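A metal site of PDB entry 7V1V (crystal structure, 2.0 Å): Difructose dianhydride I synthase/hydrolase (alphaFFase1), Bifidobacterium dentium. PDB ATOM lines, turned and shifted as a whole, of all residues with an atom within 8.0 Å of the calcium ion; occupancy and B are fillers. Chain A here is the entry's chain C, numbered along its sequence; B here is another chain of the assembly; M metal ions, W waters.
The side-chain carboxylate of Glu 270 sits close to the side-chain amide oxygen of Asn 226, 3.0 Å away. OD2 of Asp 26 of chain B lies within hydrogen-bond range of N of Asn 31 of chain B, at 3.3 Å. The side-chain amide oxygen of Asn 231 sits at hydrogen-bond distance from the side-chain amide nitrogen of Asn 31 of chain B (3.0 Å). The side-chain amide nitrogen of Asn 31 of chain B sits close to the side-chain amide nitrogen of Asn 226 (3.4 Å). OD1 of Asn 272 sits close to N of Gly 289, 3.5 Å away. The side-chain carboxylate (OE1) of Glu 343 sits at hydrogen-bond distance from the backbone NH (N) of Asn 272, 2.8 Å away. The side-chain amide nitrogen of Asn 272 is in hydrogen-bond range of the backbone carbonyl oxygen of Gly 287 (3.0 Å). The side-chain hydroxyl (OG1) of Thr 288 lies within hydrogen-bond range of the side-chain carboxylate (OD2) of Asp 292 (2.6 Å).
Five residues have an atom within 4 Å of the calcium ion: Glu 270, Asn 272, Thr 288, Asn 31 of chain B and Asp 33 of chain B.
The side-chain carboxylate (OD2) of Asp 33 of chain B binds the calcium ion. The backbone carbonyl oxygen (O) of Glu 270 binds the calcium ion (2.3 Å). The side-chain amide oxygen (OD1) of Asn 31 of chain B is bound to the calcium ion, at 2.4 Å. The side-chain amide oxygen (OD1) of Asn 272 is bound to the calcium ion (2.4 Å). Water W1 binds the calcium ion, 2.4 Å away. The calcium ion is bound by O of Thr 288.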
ATOM      1  N   ASN A 226      11.072 -16.446  19.218  1.00  0.00           N
ATOM      2  CA  ASN A 226      11.080 -17.249  20.467  1.00  0.00           C
ATOM      3  C   ASN A 226      12.152 -18.329  20.412  1.00  0.00           C
ATOM      4  O   ASN A 226      12.146 -19.152  21.306  1.00  0.00           O
ATOM      5  CB  ASN A 226       9.718 -17.830  20.823  1.00  0.00           C
ATOM      6  CG  ASN A 226       8.779 -16.806  21.406  1.00  0.00           C
ATOM      7  OD1 ASN A 226       7.568 -16.814  21.146  1.00  0.00           O
ATOM      8  ND2 ASN A 226       9.320 -15.858  22.132  1.00  0.00           N
ATOM      9  N   ASN A 231      15.507 -14.751  22.346  1.00  0.00           N
ATOM     10  CA  ASN A 231      14.937 -14.492  23.691  1.00  0.00           C
ATOM     11  C   ASN A 231      16.045 -14.117  24.692  1.00  0.00           C
ATOM     12  O   ASN A 231      15.708 -13.524  25.705  1.00  0.00           O
ATOM     13  CB  ASN A 231      14.108 -15.669  24.200  1.00  0.00           C
ATOM     14  CG  ASN A 231      12.715 -15.720  23.591  1.00  0.00           C
ATOM     15  OD1 ASN A 231      12.261 -14.768  22.973  1.00  0.00           O
ATOM     16  ND2 ASN A 231      12.075 -16.875  23.712  1.00  0.00           N
ATOM     17  N   GLY A 269       4.232 -10.467  18.463  1.00  0.00           N
ATOM     18  CA  GLY A 269       3.812  -9.724  19.675  1.00  0.00           C
ATOM     19  C   GLY A 269       4.600  -9.990  20.949  1.00  0.00           C
ATOM     20  O   GLY A 269       4.029  -9.719  22.054  1.00  0.00           O
ATOM     21  N   GLU A 270       5.871 -10.406  20.891  1.00  0.00           N
ATOM     22  CA  GLU A 270       6.652 -10.667  22.145  1.00  0.00           C
ATOM     23  C   GLU A 270       7.137  -9.363  22.810  1.00  0.00           C
ATOM     24  O   GLU A 270       7.547  -9.386  24.026  1.00  0.00           O
ATOM     25  CB  GLU A 270       7.820 -11.578  21.822  1.00  0.00           C
ATOM     26  CG  GLU A 270       7.436 -13.014  21.553  1.00  0.00           C
ATOM     27  CD  GLU A 270       6.760 -13.724  22.715  1.00  0.00           C
ATOM     28  OE1 GLU A 270       7.080 -13.399  23.871  1.00  0.00           O
ATOM     29  OE2 GLU A 270       5.947 -14.655  22.444  1.00  0.00           O
ATOM     30  N   GLY A 271       7.073  -8.275  22.064  1.00  0.00           N
ATOM     31  CA  GLY A 271       7.604  -6.976  22.481  1.00  0.00           C
ATOM     32  C   GLY A 271       6.815  -6.367  23.617  1.00  0.00           C
ATOM     33  O   GLY A 271       5.570  -6.417  23.574  1.00  0.00           O
ATOM     34  N   ASN A 272       7.528  -5.775  24.580  1.00  0.00           N
ATOM     35  CA  ASN A 272       6.965  -5.149  25.794  1.00  0.00           C
ATOM     36  C   ASN A 272       6.611  -3.693  25.477  1.00  0.00           C
ATOM     37  O   ASN A 272       7.413  -2.983  24.873  1.00  0.00           O
ATOM     38  CB  ASN A 272       7.955  -5.154  26.953  1.00  0.00           C
ATOM     39  CG  ASN A 272       8.362  -6.521  27.444  1.00  0.00           C
ATOM     40  OD1 ASN A 272       7.934  -7.542  26.899  1.00  0.00           O
ATOM     41  ND2 ASN A 272       9.251  -6.543  28.433  1.00  0.00           N
ATOM     42  N   ASP A 273       5.442  -3.248  25.911  1.00  0.00           N
ATOM     43  CA  ASP A 273       5.179  -1.798  26.125  1.00  0.00           C
ATOM     44  C   ASP A 273       6.214  -1.299  27.146  1.00  0.00           C
ATOM     45  O   ASP A 273       6.540  -2.007  28.130  1.00  0.00           O
ATOM     46  CB  ASP A 273       3.729  -1.534  26.523  1.00  0.00           C
ATOM     47  CG  ASP A 273       3.260  -2.242  27.777  1.00  0.00           C
ATOM     48  OD1 ASP A 273       3.151  -3.505  27.750  1.00  0.00           O
ATOM     49  OD2 ASP A 273       3.016  -1.522  28.769  1.00  0.00           O
ATOM     50  N   MET A 274       6.708  -0.084  26.929  1.00  0.00           N
ATOM     51  CA  MET A 274       7.620   0.617  27.847  1.00  0.00           C
ATOM     52  C   MET A 274       7.224   2.087  27.793  1.00  0.00           C
ATOM     53  O   MET A 274       7.267   2.639  26.681  1.00  0.00           O
ATOM     54  CB  MET A 274       9.089   0.462  27.462  1.00  0.00           C
ATOM     55  CG  MET A 274       9.620  -0.974  27.532  1.00  0.00           C
ATOM     56  SD  MET A 274      11.364  -1.059  27.100  1.00  0.00           S
ATOM     57  CE  MET A 274      11.670  -2.829  27.175  1.00  0.00           C
ATOM     58  N   GLY A 287       6.088  -3.270  30.539  1.00  0.00           N
ATOM     59  CA  GLY A 287       5.129  -4.323  30.199  1.00  0.00           C
ATOM     60  C   GLY A 287       5.832  -5.630  29.998  1.00  0.00           C
ATOM     61  O   GLY A 287       7.044  -5.765  30.330  1.00  0.00           O
ATOM     62  N   THR A 288       5.108  -6.592  29.442  1.00  0.00           N
ATOM     63  CA  THR A 288       5.559  -7.992  29.386  1.00  0.00           C
ATOM     64  C   THR A 288       5.426  -8.547  27.972  1.00  0.00           C
ATOM     65  O   THR A 288       6.055  -9.566  27.701  1.00  0.00           O
ATOM     66  CB  THR A 288       4.830  -8.817  30.466  1.00  0.00           C
ATOM     67  OG1 THR A 288       3.440  -8.778  30.179  1.00  0.00           O
ATOM     68  CG2 THR A 288       5.109  -8.317  31.877  1.00  0.00           C
ATOM     69  N   GLY A 289       4.506  -7.997  27.158  1.00  0.00           N
ATOM     70  CA  GLY A 289       4.339  -8.422  25.757  1.00  0.00           C
ATOM     71  C   GLY A 289       3.263  -7.595  25.091  1.00  0.00           C
ATOM     72  O   GLY A 289       2.626  -6.798  25.797  1.00  0.00           O
ATOM     73  N   THR A 290       3.072  -7.748  23.795  1.00  0.00           N
ATOM     74  CA  THR A 290       2.161  -6.840  23.035  1.00  0.00           C
ATOM     75  C   THR A 290       0.704  -7.302  23.227  1.00  0.00           C
ATOM     76  O   THR A 290      -0.133  -6.428  23.462  1.00  0.00           O
ATOM     77  CB  THR A 290       2.601  -6.679  21.569  1.00  0.00           C
ATOM     78  OG1 THR A 290       4.022  -6.475  21.464  1.00  0.00           O
ATOM     79  CG2 THR A 290       1.855  -5.518  20.927  1.00  0.00           C
ATOM     80  N   GLU A 291       0.387  -8.591  23.128  1.00  0.00           N
ATOM     81  CA  GLU A 291      -0.996  -9.044  23.441  1.00  0.00           C
ATOM     82  C   GLU A 291      -1.262  -8.748  24.928  1.00  0.00           C
ATOM     83  O   GLU A 291      -2.393  -8.237  25.253  1.00  0.00           O
ATOM     84  CB  GLU A 291      -1.278 -10.502  23.036  1.00  0.00           C
ATOM     85  CG  GLU A 291      -0.876 -11.571  24.031  1.00  0.00           C
ATOM     86  CD  GLU A 291       0.546 -12.062  23.898  1.00  0.00           C
ATOM     87  OE1 GLU A 291       1.469 -11.202  23.875  1.00  0.00           O
ATOM     88  OE2 GLU A 291       0.728 -13.293  23.794  1.00  0.00           O
ATOM     89  N   ASP A 292      -0.240  -8.910  25.775  1.00  0.00           N
ATOM     90  CA  ASP A 292      -0.312  -8.600  27.228  1.00  0.00           C
ATOM     91  C   ASP A 292      -0.768  -7.138  27.386  1.00  0.00           C
ATOM     92  O   ASP A 292      -1.714  -6.880  28.137  1.00  0.00           O
ATOM     93  CB  ASP A 292       1.048  -8.839  27.894  1.00  0.00           C
ATOM     94  CG  ASP A 292       1.592 -10.251  27.802  1.00  0.00           C
ATOM     95  OD1 ASP A 292       0.960 -11.126  27.165  1.00  0.00           O
ATOM     96  OD2 ASP A 292       2.656 -10.471  28.398  1.00  0.00           O
ATOM     97  N   GLU A 343       8.328  -2.573  22.074  1.00  0.00           N
ATOM     98  CA  GLU A 343       9.407  -3.280  21.358  1.00  0.00           C
ATOM     99  C   GLU A 343       8.764  -3.951  20.137  1.00  0.00           C
ATOM    100  O   GLU A 343       7.700  -4.573  20.320  1.00  0.00           O
ATOM    101  CB  GLU A 343      10.077  -4.388  22.166  1.00  0.00           C
ATOM    102  CG  GLU A 343      10.636  -4.002  23.508  1.00  0.00           C
ATOM    103  CD  GLU A 343      11.157  -5.242  24.232  1.00  0.00           C
ATOM    104  OE1 GLU A 343      10.295  -6.060  24.646  1.00  0.00           O
ATOM    105  OE2 GLU A 343      12.409  -5.433  24.298  1.00  0.00           O
ATOM    106  N   GLY A 345       8.563  -6.813  18.240  1.00  0.00           N
ATOM    107  CA  GLY A 345       9.128  -8.115  18.592  1.00  0.00           C
ATOM    108  C   GLY A 345      10.068  -7.974  19.787  1.00  0.00           C
ATOM    109  O   GLY A 345      10.412  -6.806  20.156  1.00  0.00           O
ATOM    110  N   HIS A 346      10.454  -9.083  20.404  1.00  0.00           N
ATOM    111  CA  HIS A 346      11.342  -9.039  21.594  1.00  0.00           C
ATOM    112  C   HIS A 346      12.622  -8.297  21.211  1.00  0.00           C
ATOM    113  O   HIS A 346      13.215  -8.634  20.202  1.00  0.00           O
ATOM    114  CB  HIS A 346      11.675 -10.425  22.162  1.00  0.00           C
ATOM    115  CG  HIS A 346      12.724 -10.308  23.214  1.00  0.00           C
ATOM    116  ND1 HIS A 346      12.539  -9.521  24.337  1.00  0.00           N
ATOM    117  CD2 HIS A 346      14.002 -10.730  23.220  1.00  0.00           C
ATOM    118  CE1 HIS A 346      13.654  -9.530  25.042  1.00  0.00           C
ATOM    119  NE2 HIS A 346      14.596 -10.262  24.360  1.00  0.00           N
ATOM    120  N   ALA A 347      12.991  -7.287  21.997  1.00  0.00           N
ATOM    121  CA  ALA A 347      14.251  -6.527  21.841  1.00  0.00           C
ATOM    122  C   ALA A 347      14.366  -5.987  20.409  1.00  0.00           C
ATOM    123  O   ALA A 347      15.506  -5.828  19.905  1.00  0.00           O
ATOM    124  CB  ALA A 347      15.423  -7.387  22.214  1.00  0.00           C
ATOM    125  N   TRP B  25       7.895  -8.225  34.391  1.00  0.00           N
ATOM    126  CA  TRP B  25       8.853  -7.894  33.308  1.00  0.00           C
ATOM    127  C   TRP B  25      10.214  -8.512  33.629  1.00  0.00           C
ATOM    128  O   TRP B  25      10.602  -8.611  34.820  1.00  0.00           O
ATOM    129  CB  TRP B  25       8.904  -6.368  33.037  1.00  0.00           C
ATOM    130  CG  TRP B  25       9.557  -5.522  34.090  1.00  0.00           C
ATOM    131  CD1 TRP B  25       9.003  -5.112  35.265  1.00  0.00           C
ATOM    132  CD2 TRP B  25      10.877  -4.929  34.039  1.00  0.00           C
ATOM    133  NE1 TRP B  25       9.889  -4.347  35.960  1.00  0.00           N
ATOM    134  CE2 TRP B  25      11.025  -4.186  35.229  1.00  0.00           C
ATOM    135  CE3 TRP B  25      11.928  -4.962  33.122  1.00  0.00           C
ATOM    136  CZ2 TRP B  25      12.202  -3.492  35.531  1.00  0.00           C
ATOM    137  CZ3 TRP B  25      13.101  -4.277  33.409  1.00  0.00           C
ATOM    138  CH2 TRP B  25      13.231  -3.560  34.605  1.00  0.00           C
ATOM    139  N   ASP B  26      10.897  -8.968  32.586  1.00  0.00           N
ATOM    140  CA  ASP B  26      12.219  -9.637  32.707  1.00  0.00           C
ATOM    141  C   ASP B  26      13.239  -8.565  33.084  1.00  0.00           C
ATOM    142  O   ASP B  26      13.575  -7.772  32.223  1.00  0.00           O
ATOM    143  CB  ASP B  26      12.587 -10.334  31.404  1.00  0.00           C
ATOM    144  CG  ASP B  26      13.734 -11.323  31.545  1.00  0.00           C
ATOM    145  OD1 ASP B  26      14.605 -11.153  32.472  1.00  0.00           O
ATOM    146  OD2 ASP B  26      13.788 -12.213  30.694  1.00  0.00           O
ATOM    147  N   GLY B  29      16.301  -7.847  31.174  1.00  0.00           N
ATOM    148  CA  GLY B  29      16.022  -7.196  29.876  1.00  0.00           C
ATOM    149  C   GLY B  29      15.746  -8.181  28.738  1.00  0.00           C
ATOM    150  O   GLY B  29      15.739  -7.757  27.562  1.00  0.00           O
ATOM    151  N   LYS B  30      15.534  -9.456  29.064  1.00  0.00           N
ATOM    152  CA  LYS B  30      15.359 -10.562  28.082  1.00  0.00           C
ATOM    153  C   LYS B  30      13.866 -10.822  27.930  1.00  0.00           C
ATOM    154  O   LYS B  30      13.081  -9.921  28.302  1.00  0.00           O
ATOM    155  CB  LYS B  30      16.193 -11.779  28.531  1.00  0.00           C
ATOM    156  CG  LYS B  30      17.693 -11.494  28.557  1.00  0.00           C
ATOM    157  CD  LYS B  30      18.560 -12.589  29.110  1.00  0.00           C
ATOM    158  CE  LYS B  30      20.020 -12.167  29.043  1.00  0.00           C
ATOM    159  NZ  LYS B  30      20.924 -13.219  29.521  1.00  0.00           N
ATOM    160  N   ASN B  31      13.468 -11.983  27.385  1.00  0.00           N
ATOM    161  CA  ASN B  31      12.030 -12.245  27.049  1.00  0.00           C
ATOM    162  C   ASN B  31      11.370 -13.261  27.998  1.00  0.00           C
ATOM    163  O   ASN B  31      10.354 -13.881  27.559  1.00  0.00           O
ATOM    164  CB  ASN B  31      11.833 -12.688  25.597  1.00  0.00           C
ATOM    165  CG  ASN B  31      10.427 -12.439  25.095  1.00  0.00           C
ATOM    166  OD1 ASN B  31       9.797 -11.446  25.457  1.00  0.00           O
ATOM    167  ND2 ASN B  31       9.904 -13.335  24.273  1.00  0.00           N
ATOM    168  N   GLN B  32      11.863 -13.423  29.235  1.00  0.00           N
ATOM    169  CA  GLN B  32      11.082 -14.141  30.291  1.00  0.00           C
ATOM    170  C   GLN B  32      10.315 -13.120  31.143  1.00  0.00           C
ATOM    171  O   GLN B  32      10.719 -12.915  32.342  1.00  0.00           O
ATOM    172  CB  GLN B  32      11.968 -15.025  31.174  1.00  0.00           C
ATOM    173  CG  GLN B  32      12.542 -16.224  30.434  1.00  0.00           C
ATOM    174  CD  GLN B  32      13.321 -17.092  31.395  1.00  0.00           C
ATOM    175  OE1 GLN B  32      13.057 -17.136  32.597  1.00  0.00           O
ATOM    176  NE2 GLN B  32      14.284 -17.817  30.855  1.00  0.00           N
ATOM    177  N   ASP B  33       9.208 -12.598  30.611  1.00  0.00           N
ATOM    178  CA  ASP B  33       8.449 -11.484  31.248  1.00  0.00           C
ATOM    179  C   ASP B  33       7.331 -12.067  32.149  1.00  0.00           C
ATOM    180  O   ASP B  33       6.224 -11.480  32.250  1.00  0.00           O
ATOM    181  CB  ASP B  33       7.948 -10.492  30.187  1.00  0.00           C
ATOM    182  CG  ASP B  33       9.061  -9.869  29.366  1.00  0.00           C
ATOM    183  OD1 ASP B  33       9.815  -9.027  29.944  1.00  0.00           O
ATOM    184  OD2 ASP B  33       9.176 -10.218  28.159  1.00  0.00           O
ATOM    185  N   TYR B  34       7.637 -13.189  32.794  1.00  0.00           N
ATOM    186  CA  TYR B  34       6.719 -13.923  33.686  1.00  0.00           C
ATOM    187  C   TYR B  34       7.522 -14.362  34.902  1.00  0.00           C
ATOM    188  O   TYR B  34       8.734 -14.452  34.761  1.00  0.00           O
ATOM    189  CB  TYR B  34       6.115 -15.136  32.969  1.00  0.00           C
ATOM    190  CG  TYR B  34       7.131 -16.140  32.465  1.00  0.00           C
ATOM    191  CD1 TYR B  34       7.688 -16.001  31.196  1.00  0.00           C
ATOM    192  CD2 TYR B  34       7.542 -17.211  33.218  1.00  0.00           C
ATOM    193  CE1 TYR B  34       8.609 -16.916  30.703  1.00  0.00           C
ATOM    194  CE2 TYR B  34       8.463 -18.128  32.754  1.00  0.00           C
ATOM    195  CZ  TYR B  34       8.990 -17.988  31.485  1.00  0.00           C
ATOM    196  OH  TYR B  34       9.922 -18.876  31.008  1.00  0.00           O
ATOM    197  N   TYR B 187       2.218 -14.170  34.552  1.00  0.00           N
ATOM    198  CA  TYR B 187       2.399 -12.858  33.895  1.00  0.00           C
ATOM    199  C   TYR B 187       1.480 -11.890  34.609  1.00  0.00           C
ATOM    200  O   TYR B 187       0.321 -12.287  34.875  1.00  0.00           O
ATOM    201  CB  TYR B 187       1.960 -12.941  32.433  1.00  0.00           C
ATOM    202  CG  TYR B 187       2.903 -13.595  31.465  1.00  0.00           C
ATOM    203  CD1 TYR B 187       2.914 -14.969  31.234  1.00  0.00           C
ATOM    204  CD2 TYR B 187       3.755 -12.822  30.708  1.00  0.00           C
ATOM    205  CE1 TYR B 187       3.745 -15.539  30.277  1.00  0.00           C
ATOM    206  CE2 TYR B 187       4.603 -13.387  29.766  1.00  0.00           C
ATOM    207  CZ  TYR B 187       4.598 -14.745  29.543  1.00  0.00           C
ATOM    208  OH  TYR B 187       5.487 -15.263  28.624  1.00  0.00           O
HETATM  209 CA    CA M   1       8.294  -9.762  26.130  1.00  0.00          CA
HETATM  210  O   HOH W   1       6.845 -11.718  25.930  1.00  0.00           O
